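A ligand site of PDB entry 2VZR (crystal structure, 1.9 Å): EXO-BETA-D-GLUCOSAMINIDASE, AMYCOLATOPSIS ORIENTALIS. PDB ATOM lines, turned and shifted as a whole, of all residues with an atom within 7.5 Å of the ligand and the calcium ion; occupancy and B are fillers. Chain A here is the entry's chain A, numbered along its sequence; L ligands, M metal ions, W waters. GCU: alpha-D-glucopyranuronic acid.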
ATOM      1  N   GLN A  15     -30.534 -13.319  30.878  1.00  0.00           N
ATOM      2  CA  GLN A  15     -29.643 -12.241  31.337  1.00  0.00           C
ATOM      3  C   GLN A  15     -28.470 -12.005  30.384  1.00  0.00           C
ATOM      4  O   GLN A  15     -27.312 -12.218  30.736  1.00  0.00           O
ATOM      5  CB  GLN A  15     -29.147 -12.516  32.741  1.00  0.00           C
ATOM      6  CG  GLN A  15     -30.260 -12.799  33.745  1.00  0.00           C
ATOM      7  CD  GLN A  15     -29.733 -12.842  35.150  1.00  0.00           C
ATOM      8  OE1 GLN A  15     -29.343 -11.821  35.704  1.00  0.00           O
ATOM      9  NE2 GLN A  15     -29.702 -14.031  35.732  1.00  0.00           N
ATOM     10  N   GLY A  16     -28.811 -11.586  29.169  1.00  0.00           N
ATOM     11  CA  GLY A  16     -27.831 -11.275  28.141  1.00  0.00           C
ATOM     12  C   GLY A  16     -28.480 -10.400  27.084  1.00  0.00           C
ATOM     13  O   GLY A  16     -29.684 -10.112  27.151  1.00  0.00           O
ATOM     14  N   GLU A  19     -25.680  -8.156  20.676  1.00  0.00           N
ATOM     15  CA  GLU A  19     -24.896  -6.970  20.358  1.00  0.00           C
ATOM     16  C   GLU A  19     -24.057  -7.253  19.135  1.00  0.00           C
ATOM     17  O   GLU A  19     -23.986  -8.391  18.668  1.00  0.00           O
ATOM     18  CB  GLU A  19     -24.068  -6.525  21.576  1.00  0.00           C
ATOM     19  CG  GLU A  19     -24.991  -6.244  22.777  1.00  0.00           C
ATOM     20  CD  GLU A  19     -24.319  -5.637  23.977  1.00  0.00           C
ATOM     21  OE1 GLU A  19     -23.086  -5.714  24.109  1.00  0.00           O
ATOM     22  OE2 GLU A  19     -25.077  -5.084  24.810  1.00  0.00           O
ATOM     23  N   ASN A  21     -21.170  -4.800  18.307  1.00  0.00           N
ATOM     24  CA  ASN A  21     -20.227  -3.669  18.342  1.00  0.00           C
ATOM     25  C   ASN A  21     -18.744  -4.057  18.312  1.00  0.00           C
ATOM     26  O   ASN A  21     -17.873  -3.195  18.366  1.00  0.00           O
ATOM     27  CB  ASN A  21     -20.525  -2.753  19.533  1.00  0.00           C
ATOM     28  CG  ASN A  21     -20.291  -3.439  20.878  1.00  0.00           C
ATOM     29  OD1 ASN A  21     -20.596  -4.616  21.043  1.00  0.00           O
ATOM     30  ND2 ASN A  21     -19.751  -2.694  21.845  1.00  0.00           N
ATOM     31  N   HIS A  22     -18.464  -5.351  18.249  1.00  0.00           N
ATOM     32  CA  HIS A  22     -17.104  -5.831  18.097  1.00  0.00           C
ATOM     33  C   HIS A  22     -17.087  -6.637  16.819  1.00  0.00           C
ATOM     34  O   HIS A  22     -17.968  -7.467  16.625  1.00  0.00           O
ATOM     35  CB  HIS A  22     -16.701  -6.717  19.286  1.00  0.00           C
ATOM     36  CG  HIS A  22     -16.672  -5.982  20.595  1.00  0.00           C
ATOM     37  ND1 HIS A  22     -15.840  -4.911  20.826  1.00  0.00           N
ATOM     38  CD2 HIS A  22     -17.366  -6.184  21.735  1.00  0.00           C
ATOM     39  CE1 HIS A  22     -16.029  -4.480  22.059  1.00  0.00           C
ATOM     40  NE2 HIS A  22     -16.951  -5.228  22.635  1.00  0.00           N
ATOM     41  N   PHE A  30     -23.807 -11.287  18.191  1.00  0.00           N
ATOM     42  CA  PHE A  30     -23.319 -12.245  19.215  1.00  0.00           C
ATOM     43  C   PHE A  30     -24.109 -12.014  20.495  1.00  0.00           C
ATOM     44  O   PHE A  30     -24.824 -11.015  20.604  1.00  0.00           O
ATOM     45  CB  PHE A  30     -21.800 -12.107  19.471  1.00  0.00           C
ATOM     46  CG  PHE A  30     -21.350 -10.699  19.783  1.00  0.00           C
ATOM     47  CD1 PHE A  30     -21.323 -10.216  21.099  1.00  0.00           C
ATOM     48  CD2 PHE A  30     -20.926  -9.853  18.755  1.00  0.00           C
ATOM     49  CE1 PHE A  30     -20.918  -8.918  21.386  1.00  0.00           C
ATOM     50  CE2 PHE A  30     -20.507  -8.536  19.017  1.00  0.00           C
ATOM     51  CZ  PHE A  30     -20.509  -8.070  20.329  1.00  0.00           C
ATOM     52  N   VAL A  31     -23.965 -12.933  21.448  1.00  0.00           N
ATOM     53  CA  VAL A  31     -24.515 -12.721  22.777  1.00  0.00           C
ATOM     54  C   VAL A  31     -23.463 -12.196  23.754  1.00  0.00           C
ATOM     55  O   VAL A  31     -22.414 -12.781  23.961  1.00  0.00           O
ATOM     56  CB  VAL A  31     -25.232 -13.974  23.366  1.00  0.00           C
ATOM     57  CG1 VAL A  31     -25.730 -13.677  24.781  1.00  0.00           C
ATOM     58  CG2 VAL A  31     -26.407 -14.332  22.503  1.00  0.00           C
ATOM     59  N   ASN A  32     -23.771 -11.032  24.315  1.00  0.00           N
ATOM     60  CA  ASN A  32     -23.062 -10.500  25.467  1.00  0.00           C
ATOM     61  C   ASN A  32     -23.780 -10.971  26.730  1.00  0.00           C
ATOM     62  O   ASN A  32     -24.900 -10.546  27.007  1.00  0.00           O
ATOM     63  CB  ASN A  32     -23.064  -8.974  25.390  1.00  0.00           C
ATOM     64  CG  ASN A  32     -22.321  -8.322  26.552  1.00  0.00           C
ATOM     65  OD1 ASN A  32     -21.870  -8.999  27.477  1.00  0.00           O
ATOM     66  ND2 ASN A  32     -22.172  -7.004  26.495  1.00  0.00           N
ATOM     67  N   TYR A  33     -23.157 -11.872  27.482  1.00  0.00           N
ATOM     68  CA  TYR A  33     -23.738 -12.325  28.754  1.00  0.00           C
ATOM     69  C   TYR A  33     -23.760 -11.156  29.750  1.00  0.00           C
ATOM     70  O   TYR A  33     -22.773 -10.438  29.863  1.00  0.00           O
ATOM     71  CB  TYR A  33     -22.894 -13.449  29.365  1.00  0.00           C
ATOM     72  CG  TYR A  33     -23.061 -14.855  28.830  1.00  0.00           C
ATOM     73  CD1 TYR A  33     -22.923 -15.135  27.468  1.00  0.00           C
ATOM     74  CD2 TYR A  33     -23.302 -15.933  29.699  1.00  0.00           C
ATOM     75  CE1 TYR A  33     -23.042 -16.426  26.987  1.00  0.00           C
ATOM     76  CE2 TYR A  33     -23.425 -17.243  29.209  1.00  0.00           C
ATOM     77  CZ  TYR A  33     -23.289 -17.475  27.852  1.00  0.00           C
ATOM     78  OH  TYR A  33     -23.412 -18.746  27.344  1.00  0.00           O
ATOM     79  N   ASP A  34     -24.832 -10.966  30.512  1.00  0.00           N
ATOM     80  CA  ASP A  34     -24.746  -9.991  31.611  1.00  0.00           C
ATOM     81  C   ASP A  34     -23.648 -10.431  32.589  1.00  0.00           C
ATOM     82  O   ASP A  34     -23.391 -11.625  32.721  1.00  0.00           O
ATOM     83  CB  ASP A  34     -26.079  -9.830  32.322  1.00  0.00           C
ATOM     84  CG  ASP A  34     -27.113  -9.155  31.477  1.00  0.00           C
ATOM     85  OD1 ASP A  34     -26.796  -8.635  30.373  1.00  0.00           O
ATOM     86  OD2 ASP A  34     -28.275  -9.142  31.938  1.00  0.00           O
ATOM     87  N   ASN A  35     -22.975  -9.476  33.242  1.00  0.00           N
ATOM     88  CA  ASN A  35     -21.880  -9.818  34.146  1.00  0.00           C
ATOM     89  C   ASN A  35     -22.423 -10.183  35.532  1.00  0.00           C
ATOM     90  O   ASN A  35     -22.279  -9.437  36.496  1.00  0.00           O
ATOM     91  CB  ASN A  35     -20.824  -8.706  34.225  1.00  0.00           C
ATOM     92  CG  ASN A  35     -20.027  -8.558  32.946  1.00  0.00           C
ATOM     93  OD1 ASN A  35     -18.795  -8.471  32.961  1.00  0.00           O
ATOM     94  ND2 ASN A  35     -20.727  -8.538  31.822  1.00  0.00           N
ATOM     95  N   VAL A  36     -23.082 -11.339  35.565  1.00  0.00           N
ATOM     96  CA  VAL A  36     -23.639 -11.941  36.779  1.00  0.00           C
ATOM     97  C   VAL A  36     -23.485 -13.449  36.615  1.00  0.00           C
ATOM     98  O   VAL A  36     -23.414 -13.956  35.491  1.00  0.00           O
ATOM     99  CB  VAL A  36     -25.161 -11.635  36.938  1.00  0.00           C
ATOM    100  CG1 VAL A  36     -25.396 -10.181  37.296  1.00  0.00           C
ATOM    101  CG2 VAL A  36     -25.945 -12.000  35.655  1.00  0.00           C
ATOM    102  N   SER A  39     -26.207 -15.995  33.966  1.00  0.00           N
ATOM    103  CA  SER A  39     -26.446 -15.646  32.574  1.00  0.00           C
ATOM    104  C   SER A  39     -26.213 -16.887  31.697  1.00  0.00           C
ATOM    105  O   SER A  39     -25.289 -17.665  31.955  1.00  0.00           O
ATOM    106  CB  SER A  39     -25.563 -14.468  32.150  1.00  0.00           C
ATOM    107  OG  SER A  39     -24.239 -14.602  32.613  1.00  0.00           O
ATOM    108  N   ALA A  60     -15.275 -14.742  22.740  1.00  0.00           N
ATOM    109  CA  ALA A  60     -14.230 -13.773  22.988  1.00  0.00           C
ATOM    110  C   ALA A  60     -14.257 -13.368  24.461  1.00  0.00           C
ATOM    111  O   ALA A  60     -15.315 -13.356  25.097  1.00  0.00           O
ATOM    112  CB  ALA A  60     -14.415 -12.536  22.074  1.00  0.00           C
ATOM    113  N   ASN A  61     -13.074 -13.024  24.973  1.00  0.00           N
ATOM    114  CA  ASN A  61     -12.880 -12.578  26.365  1.00  0.00           C
ATOM    115  C   ASN A  61     -11.727 -11.563  26.435  1.00  0.00           C
ATOM    116  O   ASN A  61     -10.555 -11.921  26.544  1.00  0.00           O
ATOM    117  CB  ASN A  61     -12.645 -13.802  27.292  1.00  0.00           C
ATOM    118  CG  ASN A  61     -12.401 -13.421  28.746  1.00  0.00           C
ATOM    119  OD1 ASN A  61     -12.472 -12.247  29.138  1.00  0.00           O
ATOM    120  ND2 ASN A  61     -12.119 -14.431  29.580  1.00  0.00           N
ATOM    121  N   GLY A  62     -12.087 -10.283  26.325  1.00  0.00           N
ATOM    122  CA  GLY A  62     -11.119  -9.191  26.357  1.00  0.00           C
ATOM    123  C   GLY A  62     -10.775  -8.747  27.764  1.00  0.00           C
ATOM    124  O   GLY A  62     -10.756  -7.553  28.060  1.00  0.00           O
ATOM    125  N   THR A  63     -10.539  -9.736  28.646  1.00  0.00           N
ATOM    126  CA  THR A  63     -10.054  -9.518  30.012  1.00  0.00           C
ATOM    127  C   THR A  63      -9.017 -10.588  30.362  1.00  0.00           C
ATOM    128  O   THR A  63      -8.874 -11.570  29.635  1.00  0.00           O
ATOM    129  CB  THR A  63     -11.182  -9.574  31.077  1.00  0.00           C
ATOM    130  OG1 THR A  63     -11.551 -10.953  31.327  1.00  0.00           O
ATOM    131  CG2 THR A  63     -12.395  -8.729  30.669  1.00  0.00           C
ATOM    132  N   ARG A  67     -13.567 -16.905  32.261  1.00  0.00           N
ATOM    133  CA  ARG A  67     -14.989 -16.846  32.509  1.00  0.00           C
ATOM    134  C   ARG A  67     -15.619 -18.219  32.241  1.00  0.00           C
ATOM    135  O   ARG A  67     -15.985 -18.542  31.111  1.00  0.00           O
ATOM    136  CB  ARG A  67     -15.615 -15.758  31.657  1.00  0.00           C
ATOM    137  CG  ARG A  67     -15.104 -14.382  32.071  1.00  0.00           C
ATOM    138  CD  ARG A  67     -16.000 -13.348  31.552  1.00  0.00           C
ATOM    139  NE  ARG A  67     -15.568 -11.994  31.899  1.00  0.00           N
ATOM    140  CZ  ARG A  67     -16.129 -10.909  31.375  1.00  0.00           C
ATOM    141  NH1 ARG A  67     -17.094 -11.033  30.466  1.00  0.00           N
ATOM    142  NH2 ARG A  67     -15.716  -9.702  31.738  1.00  0.00           N
ATOM    143  N   TRP A  90     -11.793  -8.053  22.461  1.00  0.00           N
ATOM    144  CA  TRP A  90     -13.139  -8.551  22.195  1.00  0.00           C
ATOM    145  C   TRP A  90     -13.386  -8.988  20.734  1.00  0.00           C
ATOM    146  O   TRP A  90     -14.127  -9.942  20.525  1.00  0.00           O
ATOM    147  CB  TRP A  90     -14.178  -7.557  22.694  1.00  0.00           C
ATOM    148  CG  TRP A  90     -14.135  -7.344  24.189  1.00  0.00           C
ATOM    149  CD1 TRP A  90     -13.613  -6.257  24.842  1.00  0.00           C
ATOM    150  CD2 TRP A  90     -14.601  -8.243  25.199  1.00  0.00           C
ATOM    151  NE1 TRP A  90     -13.756  -6.417  26.204  1.00  0.00           N
ATOM    152  CE2 TRP A  90     -14.336  -7.626  26.453  1.00  0.00           C
ATOM    153  CE3 TRP A  90     -15.209  -9.507  25.182  1.00  0.00           C
ATOM    154  CZ2 TRP A  90     -14.667  -8.241  27.674  1.00  0.00           C
ATOM    155  CZ3 TRP A  90     -15.552 -10.115  26.402  1.00  0.00           C
ATOM    156  CH2 TRP A  90     -15.284  -9.481  27.623  1.00  0.00           C
ATOM    157  N   ASN A 117     -18.544 -12.661  37.004  1.00  0.00           N
ATOM    158  CA  ASN A 117     -18.141 -11.959  35.772  1.00  0.00           C
ATOM    159  C   ASN A 117     -18.959 -12.324  34.543  1.00  0.00           C
ATOM    160  O   ASN A 117     -18.764 -11.757  33.475  1.00  0.00           O
ATOM    161  CB  ASN A 117     -16.647 -12.181  35.505  1.00  0.00           C
ATOM    162  CG  ASN A 117     -15.779 -11.433  36.497  1.00  0.00           C
ATOM    163  OD1 ASN A 117     -15.981 -10.245  36.741  1.00  0.00           O
ATOM    164  ND2 ASN A 117     -14.804 -12.120  37.070  1.00  0.00           N
ATOM    165  N   GLY A 118     -19.890 -13.272  34.716  1.00  0.00           N
ATOM    166  CA  GLY A 118     -20.705 -13.732  33.605  1.00  0.00           C
ATOM    167  C   GLY A 118     -19.901 -14.546  32.596  1.00  0.00           C
ATOM    168  O   GLY A 118     -18.850 -15.096  32.936  1.00  0.00           O
ATOM    169  N   GLY A 119     -20.401 -14.624  31.374  1.00  0.00           N
ATOM    170  CA  GLY A 119     -19.776 -15.429  30.348  1.00  0.00           C
ATOM    171  C   GLY A 119     -18.885 -14.624  29.425  1.00  0.00           C
ATOM    172  O   GLY A 119     -18.893 -13.377  29.453  1.00  0.00           O
ATOM    173  N   PRO A 120     -18.103 -15.321  28.578  1.00  0.00           N
ATOM    174  CA  PRO A 120     -17.433 -14.658  27.489  1.00  0.00           C
ATOM    175  C   PRO A 120     -18.550 -14.168  26.571  1.00  0.00           C
ATOM    176  O   PRO A 120     -19.701 -14.593  26.755  1.00  0.00           O
ATOM    177  CB  PRO A 120     -16.645 -15.798  26.827  1.00  0.00           C
ATOM    178  CG  PRO A 120     -17.422 -17.025  27.141  1.00  0.00           C
ATOM    179  CD  PRO A 120     -17.917 -16.788  28.543  1.00  0.00           C
ATOM    180  N   ASN A 121     -18.247 -13.271  25.623  1.00  0.00           N
ATOM    181  CA  ASN A 121     -19.182 -13.000  24.541  1.00  0.00           C
ATOM    182  C   ASN A 121     -19.160 -14.268  23.691  1.00  0.00           C
ATOM    183  O   ASN A 121     -18.092 -14.851  23.478  1.00  0.00           O
ATOM    184  CB  ASN A 121     -18.733 -11.807  23.692  1.00  0.00           C
ATOM    185  CG  ASN A 121     -18.895 -10.462  24.401  1.00  0.00           C
ATOM    186  OD1 ASN A 121     -19.529 -10.376  25.458  1.00  0.00           O
ATOM    187  ND2 ASN A 121     -18.326  -9.413  23.804  1.00  0.00           N
HETATM  188  C1  GCU L   1     -17.049  -4.715  27.567  1.00  0.00           C
HETATM  189  C2  GCU L   1     -17.271  -5.336  26.181  1.00  0.00           C
HETATM  190  C3  GCU L   1     -18.462  -6.287  26.221  1.00  0.00           C
HETATM  191  C4  GCU L   1     -18.217  -7.347  27.275  1.00  0.00           C
HETATM  192  C5  GCU L   1     -17.994  -6.700  28.650  1.00  0.00           C
HETATM  193  C6  GCU L   1     -17.659  -7.749  29.714  1.00  0.00           C
HETATM  194  O1  GCU L   1     -18.136  -3.858  27.860  1.00  0.00           O
HETATM  195  O2  GCU L   1     -17.491  -4.339  25.193  1.00  0.00           O
HETATM  196  O3  GCU L   1     -18.645  -6.894  24.955  1.00  0.00           O
HETATM  197  O4  GCU L   1     -19.302  -8.252  27.281  1.00  0.00           O
HETATM  198  O5  GCU L   1     -16.940  -5.727  28.570  1.00  0.00           O
HETATM  199  O6A GCU L   1     -18.375  -8.769  29.864  1.00  0.00           O
HETATM  200  O6B GCU L   1     -16.626  -7.568  30.400  1.00  0.00           O
HETATM  201 CA    CA M   1     -20.852  -9.172  29.543  1.00  0.00          CA
HETATM  202  O   HOH W   1     -17.368  -1.856  29.443  1.00  0.00           O
HETATM  203  O   HOH W   2     -14.647  -5.567  30.455  1.00  0.00           O
HETATM  204  O   HOH W   3     -15.119  -2.566  24.853  1.00  0.00           O
HETATM  205  O   HOH W   4     -21.228  -4.449  28.180  1.00  0.00           O
HETATM  206  O   HOH W   5     -20.018 -11.263  30.979  1.00  0.00           O
HETATM  207  O   HOH W   6     -20.684  -5.969  23.261  1.00  0.00           O
HETATM  208  O   HOH W   7     -20.088 -11.344  27.810  1.00  0.00           O
HETATM  209  O   HOH W   8     -21.692  -7.157  29.785  1.00  0.00           O
HETATM  210  O   HOH W   9     -19.764  -2.844  25.065  1.00  0.00           O
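Within 4 Å of the calcium ion: Asn 32, Tyr 33 and Asn 35.
Water W5 lies within hydrogen-bond range of O of Asn 117 (2.8 Å), O of Gly 119 (2.8 Å) and NH1 of Arg 67 (3.0 Å).
Water W9 bridges O2 of the ligand (2.7 Å) and ND2 of Asn 21 (3.2 Å).
Water W6 lies within hydrogen-bond range of the side-chain carboxylate of Glu 19, the side-chain amide oxygen of Asn 21 and an oxygen (O3) of the ligand.
Water W4 lies within hydrogen-bond range of O1 of the ligand (3.2 Å) and ND2 of Asn 32 (3.2 Å).
The calcium ion is bound by water W8 (2.2 Å), OD1 of Asn 32 (2.3 Å), O of Tyr 33 (2.3 Å), ND2 of Asn 35 (2.4 Å), O6A of the ligand (2.5 Å), water W5 (2.7 Å), water W7 (2.9 Å) and O4 of the ligand (2.9 Å).
The calcium ion has eight donor atoms within binding distance.
ND2 of Asn 121 sits at hydrogen-bond distance from O3 of the ligand, at 2.8 Å.
O2 of the ligand sits at hydrogen-bond distance from NE2 of His 22 (2.8 Å).
The guanidinium group (NH2) of Arg 67 lies within salt-bridge range of an oxygen (O6B) of the ligand (2.7 Å).
Trp 90 touches the ligand.
Hydrophobic or aromatic side chains that line the ligand: His 22 and Trp 90.
Of the 24 residues printed, 6 come within 4 Å of the ligand.
The nearest printed residue that does not touch the ligand is Asn 21 (4.4 Å).
NH1 of Arg 67 sits at hydrogen-bond distance from O of Gly 119, 3.1 Å away.
OD1 of Asn 35 lies close to O of Asn 117 (3.3 Å).
The side-chain amide oxygen of Asn 32 lies close to the side-chain amide oxygen of Asn 121, 3.4 Å away.
The side-chain carboxylate (OE1) of Glu 19 lies within hydrogen-bond range of the side-chain amide nitrogen (ND2) of Asn 32 (2.9 Å).
O of Asn 121 is in hydrogen-bond range of N of Ala 60 (2.9 Å).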
